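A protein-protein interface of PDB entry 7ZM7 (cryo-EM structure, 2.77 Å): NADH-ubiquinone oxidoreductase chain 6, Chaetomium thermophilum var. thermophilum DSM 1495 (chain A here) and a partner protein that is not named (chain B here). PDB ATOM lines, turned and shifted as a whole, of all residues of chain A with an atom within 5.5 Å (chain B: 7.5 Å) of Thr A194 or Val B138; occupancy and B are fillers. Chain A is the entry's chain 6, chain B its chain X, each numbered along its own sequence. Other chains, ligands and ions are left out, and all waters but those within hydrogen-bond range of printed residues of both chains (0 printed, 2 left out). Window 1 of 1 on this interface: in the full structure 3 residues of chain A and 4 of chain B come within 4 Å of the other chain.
Thr A194 touches Met B135 (CG2 to CE, 3.7 Å).
Val B138 touches Thr A194 (CG1 to C, 3.8 Å).
OD1 of Asn A195 touches CG2 of Val B138, at 3.4 Å.
The guanidinium group (NH1) of Arg B141 is in hydrogen-bond range of the side-chain amide oxygen (OD1) of Asn A195 (3.4 Å).
The side-chain amide nitrogen (NE2) of Gln B142 sits at hydrogen-bond distance from the side-chain amide oxygen (OD1) of Asn A197.
Of chain B, only Met B135 and Val B138 come within 4 Å of Thr A194.
Printed residues of chain B within 4 Å of Asn A195: Val B138 (3.4 Å) and Arg B141 (3.4 Å).
Of the printed residues of chain B, Asn A197 touches Gln B142 (3.1 Å).
Val B138 touches just these residues of chain A: Thr A194 and Asn A195.
Printed residues of chain A within 4 Å of Arg B141: Asn A195.
Of the printed residues of chain A, Gln B142 touches Asn A197.
Arg B144 touches none of the printed residues of chain A.
Trp B155 touches none of the printed residues of chain A.
The nearest residue of chain B that does not touch Thr A194 is Gln B142 (4.9 Å).
OG1 of Thr A194 is in hydrogen-bond range of O of Asn A190.
The backbone carbonyl oxygen (O) of Thr A194 lies close to the side-chain amide nitrogen (ND2) of Asn A197.
NH2 of Arg B141 sits at hydrogen-bond distance from O of Gly B137 (3.1 Å).
ND2 of Asn A195 sits at hydrogen-bond distance from OG1 of Thr A194 (3.1 Å).
Hydrophobic or aromatic side chains of chain B that line the printed part of chain A: Met B135 and Val B138.
Among the printed residues, 5 pairs touch across the chains.
Among the printed residues, no Asp or Glu carboxylate lies within 4 Å of a Lys or Arg side-chain nitrogen of the other chain.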
ATOM      1  N   GLY A 189      40.691  -8.269   7.707  1.00  0.00           N
ATOM      2  CA  GLY A 189      39.321  -8.793   7.807  1.00  0.00           C
ATOM      3  C   GLY A 189      38.424  -7.968   8.700  1.00  0.00           C
ATOM      4  O   GLY A 189      37.259  -7.819   8.336  1.00  0.00           O
ATOM      5  N   ASN A 190      38.959  -7.401   9.783  1.00  0.00           N
ATOM      6  CA  ASN A 190      38.169  -6.594  10.746  1.00  0.00           C
ATOM      7  C   ASN A 190      37.550  -5.411  10.003  1.00  0.00           C
ATOM      8  O   ASN A 190      36.515  -4.927  10.453  1.00  0.00           O
ATOM      9  CB  ASN A 190      39.005  -6.091  11.925  1.00  0.00           C
ATOM     10  CG  ASN A 190      39.528  -7.174  12.842  1.00  0.00           C
ATOM     11  OD1 ASN A 190      38.969  -8.265  12.919  1.00  0.00           O
ATOM     12  ND2 ASN A 190      40.608  -6.879  13.546  1.00  0.00           N
ATOM     13  N   ILE A 191      38.163  -4.960   8.910  1.00  0.00           N
ATOM     14  CA  ILE A 191      37.652  -3.750   8.207  1.00  0.00           C
ATOM     15  C   ILE A 191      37.236  -4.060   6.757  1.00  0.00           C
ATOM     16  O   ILE A 191      36.458  -3.269   6.207  1.00  0.00           O
ATOM     17  CB  ILE A 191      38.694  -2.615   8.312  1.00  0.00           C
ATOM     18  CG1 ILE A 191      39.955  -2.929   7.509  1.00  0.00           C
ATOM     19  CG2 ILE A 191      39.012  -2.291   9.760  1.00  0.00           C
ATOM     20  CD1 ILE A 191      40.681  -1.709   7.026  1.00  0.00           C
ATOM     21  N   MET A 192      37.705  -5.161   6.163  1.00  0.00           N
ATOM     22  CA  MET A 192      37.442  -5.438   4.757  1.00  0.00           C
ATOM     23  C   MET A 192      35.962  -5.682   4.476  1.00  0.00           C
ATOM     24  O   MET A 192      35.494  -5.454   3.355  1.00  0.00           O
ATOM     25  CB  MET A 192      38.287  -6.636   4.333  1.00  0.00           C
ATOM     26  CG  MET A 192      37.815  -7.415   3.150  1.00  0.00           C
ATOM     27  SD  MET A 192      38.962  -8.696   2.668  1.00  0.00           S
ATOM     28  CE  MET A 192      38.462  -8.852   0.967  1.00  0.00           C
ATOM     29  N   TYR A 193      35.211  -6.157   5.472  1.00  0.00           N
ATOM     30  CA  TYR A 193      33.802  -6.543   5.209  1.00  0.00           C
ATOM     31  C   TYR A 193      32.818  -5.581   5.870  1.00  0.00           C
ATOM     32  O   TYR A 193      31.620  -5.792   5.734  1.00  0.00           O
ATOM     33  CB  TYR A 193      33.553  -7.982   5.665  1.00  0.00           C
ATOM     34  CG  TYR A 193      34.559  -8.976   5.157  1.00  0.00           C
ATOM     35  CD1 TYR A 193      34.375  -9.626   3.950  1.00  0.00           C
ATOM     36  CD2 TYR A 193      35.701  -9.254   5.882  1.00  0.00           C
ATOM     37  CE1 TYR A 193      35.304 -10.532   3.475  1.00  0.00           C
ATOM     38  CE2 TYR A 193      36.645 -10.148   5.419  1.00  0.00           C
ATOM     39  CZ  TYR A 193      36.441 -10.793   4.215  1.00  0.00           C
ATOM     40  OH  TYR A 193      37.366 -11.687   3.777  1.00  0.00           O
ATOM     41  N   THR A 194      33.305  -4.557   6.564  1.00  0.00           N
ATOM     42  CA  THR A 194      32.395  -3.643   7.313  1.00  0.00           C
ATOM     43  C   THR A 194      32.599  -2.195   6.891  1.00  0.00           C
ATOM     44  O   THR A 194      31.796  -1.716   6.111  1.00  0.00           O
ATOM     45  CB  THR A 194      32.581  -3.824   8.823  1.00  0.00           C
ATOM     46  OG1 THR A 194      33.977  -3.791   9.113  1.00  0.00           O
ATOM     47  CG2 THR A 194      31.991  -5.117   9.340  1.00  0.00           C
ATOM     48  N   ASN A 195      33.653  -1.549   7.376  1.00  0.00           N
ATOM     49  CA  ASN A 195      33.958  -0.116   7.135  1.00  0.00           C
ATOM     50  C   ASN A 195      34.214   0.221   5.670  1.00  0.00           C
ATOM     51  O   ASN A 195      33.736   1.266   5.230  1.00  0.00           O
ATOM     52  CB  ASN A 195      35.220   0.252   7.911  1.00  0.00           C
ATOM     53  CG  ASN A 195      35.098   0.189   9.417  1.00  0.00           C
ATOM     54  OD1 ASN A 195      35.175   1.216  10.082  1.00  0.00           O
ATOM     55  ND2 ASN A 195      34.946  -1.003   9.967  1.00  0.00           N
ATOM     56  N   TYR A 196      34.955  -0.608   4.955  1.00  0.00           N
ATOM     57  CA  TYR A 196      35.320  -0.318   3.548  1.00  0.00           C
ATOM     58  C   TYR A 196      34.622  -1.331   2.637  1.00  0.00           C
ATOM     59  O   TYR A 196      35.199  -1.668   1.600  1.00  0.00           O
ATOM     60  CB  TYR A 196      36.839  -0.245   3.404  1.00  0.00           C
ATOM     61  CG  TYR A 196      37.542   0.803   4.228  1.00  0.00           C
ATOM     62  CD1 TYR A 196      37.975   0.532   5.516  1.00  0.00           C
ATOM     63  CD2 TYR A 196      37.793   2.060   3.713  1.00  0.00           C
ATOM     64  CE1 TYR A 196      38.618   1.490   6.277  1.00  0.00           C
ATOM     65  CE2 TYR A 196      38.442   3.029   4.457  1.00  0.00           C
ATOM     66  CZ  TYR A 196      38.854   2.744   5.745  1.00  0.00           C
ATOM     67  OH  TYR A 196      39.492   3.699   6.477  1.00  0.00           O
ATOM     68  N   ASN A 197      33.419  -1.786   3.003  1.00  0.00           N
ATOM     69  CA  ASN A 197      32.719  -2.865   2.248  1.00  0.00           C
ATOM     70  C   ASN A 197      32.278  -2.433   0.848  1.00  0.00           C
ATOM     71  O   ASN A 197      31.940  -3.322   0.061  1.00  0.00           O
ATOM     72  CB  ASN A 197      31.579  -3.501   3.053  1.00  0.00           C
ATOM     73  CG  ASN A 197      30.454  -2.557   3.420  1.00  0.00           C
ATOM     74  OD1 ASN A 197      30.448  -1.393   3.032  1.00  0.00           O
ATOM     75  ND2 ASN A 197      29.491  -3.057   4.176  1.00  0.00           N
ATOM     76  N   ASP B  26      19.155   8.317   9.808  1.00  0.00           N
ATOM     77  CA  ASP B  26      19.245   6.881   9.571  1.00  0.00           C
ATOM     78  C   ASP B  26      18.086   6.197  10.254  1.00  0.00           C
ATOM     79  O   ASP B  26      18.253   5.529  11.276  1.00  0.00           O
ATOM     80  CB  ASP B  26      20.577   6.332  10.075  1.00  0.00           C
ATOM     81  CG  ASP B  26      21.021   5.143   9.304  1.00  0.00           C
ATOM     82  OD1 ASP B  26      20.463   4.928   8.216  1.00  0.00           O
ATOM     83  OD2 ASP B  26      21.936   4.436   9.755  1.00  0.00           O
ATOM     84  N   LEU B 131      24.830  -5.552  18.270  1.00  0.00           N
ATOM     85  CA  LEU B 131      26.141  -5.241  17.674  1.00  0.00           C
ATOM     86  C   LEU B 131      26.925  -4.417  18.674  1.00  0.00           C
ATOM     87  O   LEU B 131      26.319  -3.883  19.603  1.00  0.00           O
ATOM     88  CB  LEU B 131      25.879  -4.394  16.424  1.00  0.00           C
ATOM     89  CG  LEU B 131      25.878  -5.129  15.087  1.00  0.00           C
ATOM     90  CD1 LEU B 131      24.733  -6.122  15.015  1.00  0.00           C
ATOM     91  CD2 LEU B 131      25.784  -4.136  13.943  1.00  0.00           C
ATOM     92  N   SER B 132      28.226  -4.303  18.459  1.00  0.00           N
ATOM     93  CA  SER B 132      29.143  -3.568  19.369  1.00  0.00           C
ATOM     94  C   SER B 132      28.914  -2.065  19.227  1.00  0.00           C
ATOM     95  O   SER B 132      28.489  -1.651  18.148  1.00  0.00           O
ATOM     96  CB  SER B 132      30.539  -3.905  18.962  1.00  0.00           C
ATOM     97  OG  SER B 132      31.440  -2.868  19.298  1.00  0.00           O
ATOM     98  N   PRO B 133      29.268  -1.206  20.202  1.00  0.00           N
ATOM     99  CA  PRO B 133      29.125   0.235  19.983  1.00  0.00           C
ATOM    100  C   PRO B 133      29.910   0.638  18.734  1.00  0.00           C
ATOM    101  O   PRO B 133      29.415   1.451  18.003  1.00  0.00           O
ATOM    102  CB  PRO B 133      29.667   0.817  21.279  1.00  0.00           C
ATOM    103  CG  PRO B 133      29.410  -0.262  22.303  1.00  0.00           C
ATOM    104  CD  PRO B 133      29.659  -1.557  21.566  1.00  0.00           C
ATOM    105  N   ALA B 134      31.088   0.070  18.514  1.00  0.00           N
ATOM    106  CA  ALA B 134      31.898   0.327  17.299  1.00  0.00           C
ATOM    107  C   ALA B 134      31.251  -0.204  16.015  1.00  0.00           C
ATOM    108  O   ALA B 134      31.351   0.505  15.000  1.00  0.00           O
ATOM    109  CB  ALA B 134      33.241  -0.279  17.496  1.00  0.00           C
ATOM    110  N   MET B 135      30.641  -1.396  16.030  1.00  0.00           N
ATOM    111  CA  MET B 135      29.935  -1.875  14.811  1.00  0.00           C
ATOM    112  C   MET B 135      28.673  -1.040  14.585  1.00  0.00           C
ATOM    113  O   MET B 135      28.272  -0.887  13.437  1.00  0.00           O
ATOM    114  CB  MET B 135      29.613  -3.369  14.859  1.00  0.00           C
ATOM    115  CG  MET B 135      30.793  -4.235  14.509  1.00  0.00           C
ATOM    116  SD  MET B 135      31.488  -3.789  12.909  1.00  0.00           S
ATOM    117  CE  MET B 135      32.943  -4.835  12.885  1.00  0.00           C
ATOM    118  N   GLN B 136      28.049  -0.570  15.656  1.00  0.00           N
ATOM    119  CA  GLN B 136      26.891   0.349  15.539  1.00  0.00           C
ATOM    120  C   GLN B 136      27.351   1.644  14.856  1.00  0.00           C
ATOM    121  O   GLN B 136      26.599   2.167  14.014  1.00  0.00           O
ATOM    122  CB  GLN B 136      26.316   0.643  16.913  1.00  0.00           C
ATOM    123  CG  GLN B 136      25.600  -0.532  17.551  1.00  0.00           C
ATOM    124  CD  GLN B 136      25.281  -0.238  18.995  1.00  0.00           C
ATOM    125  OE1 GLN B 136      24.736   0.808  19.326  1.00  0.00           O
ATOM    126  NE2 GLN B 136      25.624  -1.166  19.871  1.00  0.00           N
ATOM    127  N   GLY B 137      28.567   2.102  15.155  1.00  0.00           N
ATOM    128  CA  GLY B 137      29.035   3.325  14.504  1.00  0.00           C
ATOM    129  C   GLY B 137      29.415   3.086  13.065  1.00  0.00           C
ATOM    130  O   GLY B 137      29.248   4.007  12.276  1.00  0.00           O
ATOM    131  N   VAL B 138      29.889   1.896  12.723  1.00  0.00           N
ATOM    132  CA  VAL B 138      30.145   1.593  11.295  1.00  0.00           C
ATOM    133  C   VAL B 138      28.817   1.523  10.554  1.00  0.00           C
ATOM    134  O   VAL B 138      28.714   2.110   9.473  1.00  0.00           O
ATOM    135  CB  VAL B 138      31.005   0.324  11.132  1.00  0.00           C
ATOM    136  CG1 VAL B 138      31.206  -0.061   9.677  1.00  0.00           C
ATOM    137  CG2 VAL B 138      32.333   0.431  11.855  1.00  0.00           C
ATOM    138  N   ALA B 139      27.858   0.791  11.099  1.00  0.00           N
ATOM    139  CA  ALA B 139      26.530   0.669  10.468  1.00  0.00           C
ATOM    140  C   ALA B 139      25.961   2.063  10.200  1.00  0.00           C
ATOM    141  O   ALA B 139      25.550   2.320   9.072  1.00  0.00           O
ATOM    142  CB  ALA B 139      25.632  -0.158  11.358  1.00  0.00           C
ATOM    143  N   ALA B 140      25.962   2.932  11.203  1.00  0.00           N
ATOM    144  CA  ALA B 140      25.375   4.285  11.089  1.00  0.00           C
ATOM    145  C   ALA B 140      26.059   5.097   9.999  1.00  0.00           C
ATOM    146  O   ALA B 140      25.350   5.873   9.353  1.00  0.00           O
ATOM    147  CB  ALA B 140      25.498   4.999  12.402  1.00  0.00           C
ATOM    148  N   ARG B 141      27.368   4.960   9.838  1.00  0.00           N
ATOM    149  CA  ARG B 141      28.071   5.799   8.843  1.00  0.00           C
ATOM    150  C   ARG B 141      27.720   5.286   7.444  1.00  0.00           C
ATOM    151  O   ARG B 141      27.677   6.098   6.516  1.00  0.00           O
ATOM    152  CB  ARG B 141      29.553   5.905   9.202  1.00  0.00           C
ATOM    153  CG  ARG B 141      29.801   6.613  10.523  1.00  0.00           C
ATOM    154  CD  ARG B 141      31.271   6.809  10.822  1.00  0.00           C
ATOM    155  NE  ARG B 141      32.088   5.629  10.597  1.00  0.00           N
ATOM    156  CZ  ARG B 141      32.466   4.789  11.546  1.00  0.00           C
ATOM    157  NH1 ARG B 141      33.219   3.745  11.249  1.00  0.00           N
ATOM    158  NH2 ARG B 141      32.098   5.002  12.793  1.00  0.00           N
ATOM    159  N   GLN B 142      27.498   3.985   7.302  1.00  0.00           N
ATOM    160  CA  GLN B 142      27.079   3.378   6.016  1.00  0.00           C
ATOM    161  C   GLN B 142      25.662   3.792   5.601  1.00  0.00           C
ATOM    162  O   GLN B 142      25.463   3.993   4.397  1.00  0.00           O
ATOM    163  CB  GLN B 142      27.183   1.860   6.116  1.00  0.00           C
ATOM    164  CG  GLN B 142      26.684   1.114   4.888  1.00  0.00           C
ATOM    165  CD  GLN B 142      27.779   0.679   3.946  1.00  0.00           C
ATOM    166  OE1 GLN B 142      28.804   1.334   3.800  1.00  0.00           O
ATOM    167  NE2 GLN B 142      27.560  -0.435   3.274  1.00  0.00           N
ATOM    168  N   SER B 143      24.724   3.927   6.539  1.00  0.00           N
ATOM    169  CA  SER B 143      23.309   4.118   6.134  1.00  0.00           C
ATOM    170  C   SER B 143      22.810   5.562   6.229  1.00  0.00           C
ATOM    171  O   SER B 143      21.699   5.827   5.747  1.00  0.00           O
ATOM    172  CB  SER B 143      22.443   3.144   6.874  1.00  0.00           C
ATOM    173  OG  SER B 143      21.227   2.912   6.179  1.00  0.00           O
ATOM    174  N   ARG B 144      23.597   6.462   6.805  1.00  0.00           N
ATOM    175  CA  ARG B 144      23.164   7.865   6.966  1.00  0.00           C
ATOM    176  C   ARG B 144      22.927   8.447   5.562  1.00  0.00           C
ATOM    177  O   ARG B 144      23.867   8.384   4.764  1.00  0.00           O
ATOM    178  CB  ARG B 144      24.279   8.553   7.757  1.00  0.00           C
ATOM    179  CG  ARG B 144      23.953   9.937   8.287  1.00  0.00           C
ATOM    180  CD  ARG B 144      25.140  10.835   8.050  1.00  0.00           C
ATOM    181  NE  ARG B 144      25.296  10.780   6.614  1.00  0.00           N
ATOM    182  CZ  ARG B 144      26.356  11.170   5.933  1.00  0.00           C
ATOM    183  NH1 ARG B 144      27.413  11.663   6.548  1.00  0.00           N
ATOM    184  NH2 ARG B 144      26.350  11.052   4.625  1.00  0.00           N
ATOM    185  N   TRP B 155      20.494   0.112  -0.033  1.00  0.00           N
ATOM    186  CA  TRP B 155      20.955  -0.112   1.361  1.00  0.00           C
ATOM    187  C   TRP B 155      19.777   0.101   2.294  1.00  0.00           C
ATOM    188  O   TRP B 155      18.956   0.939   1.953  1.00  0.00           O
ATOM    189  CB  TRP B 155      22.165   0.752   1.765  1.00  0.00           C
ATOM    190  CG  TRP B 155      22.878   0.118   2.920  1.00  0.00           C
ATOM    191  CD1 TRP B 155      22.727   0.409   4.244  1.00  0.00           C
ATOM    192  CD2 TRP B 155      23.776  -1.002   2.858  1.00  0.00           C
ATOM    193  NE1 TRP B 155      23.487  -0.435   5.006  1.00  0.00           N
ATOM    194  CE2 TRP B 155      24.142  -1.311   4.184  1.00  0.00           C
ATOM    195  CE3 TRP B 155      24.316  -1.764   1.816  1.00  0.00           C
ATOM    196  CZ2 TRP B 155      25.011  -2.357   4.489  1.00  0.00           C
ATOM    197  CZ3 TRP B 155      25.184  -2.790   2.116  1.00  0.00           C
ATOM    198  CH2 TRP B 155      25.524  -3.082   3.436  1.00  0.00           C
ATOM    199  N   HIS B 161      21.262   1.518  16.293  1.00  0.00           N
ATOM    200  CA  HIS B 161      22.327   2.425  16.761  1.00  0.00           C
ATOM    201  C   HIS B 161      21.692   3.660  17.385  1.00  0.00           C
ATOM    202  O   HIS B 161      20.488   3.863  17.198  1.00  0.00           O
ATOM    203  CB  HIS B 161      23.280   2.740  15.608  1.00  0.00           C
ATOM    204  CG  HIS B 161      22.610   3.305  14.408  1.00  0.00           C
ATOM    205  ND1 HIS B 161      22.397   4.653  14.253  1.00  0.00           N
ATOM    206  CD2 HIS B 161      22.109   2.711  13.307  1.00  0.00           C
ATOM    207  CE1 HIS B 161      21.782   4.868  13.113  1.00  0.00           C
ATOM    208  NE2 HIS B 161      21.599   3.695  12.515  1.00  0.00           N
ATOM    209  N   GLN B 163      23.083   6.791  16.694  1.00  0.00           N
ATOM    210  CA  GLN B 163      23.627   7.944  15.922  1.00  0.00           C
ATOM    211  C   GLN B 163      22.647   8.334  14.814  1.00  0.00           C
ATOM    212  O   GLN B 163      22.745   7.761  13.725  1.00  0.00           O
ATOM    213  CB  GLN B 163      25.011   7.562  15.417  1.00  0.00           C
ATOM    214  CG  GLN B 163      25.855   6.979  16.534  1.00  0.00           C
ATOM    215  CD  GLN B 163      26.865   5.977  16.044  1.00  0.00           C
ATOM    216  OE1 GLN B 163      27.301   6.032  14.902  1.00  0.00           O
ATOM    217  NE2 GLN B 163      27.243   5.056  16.915  1.00  0.00           N
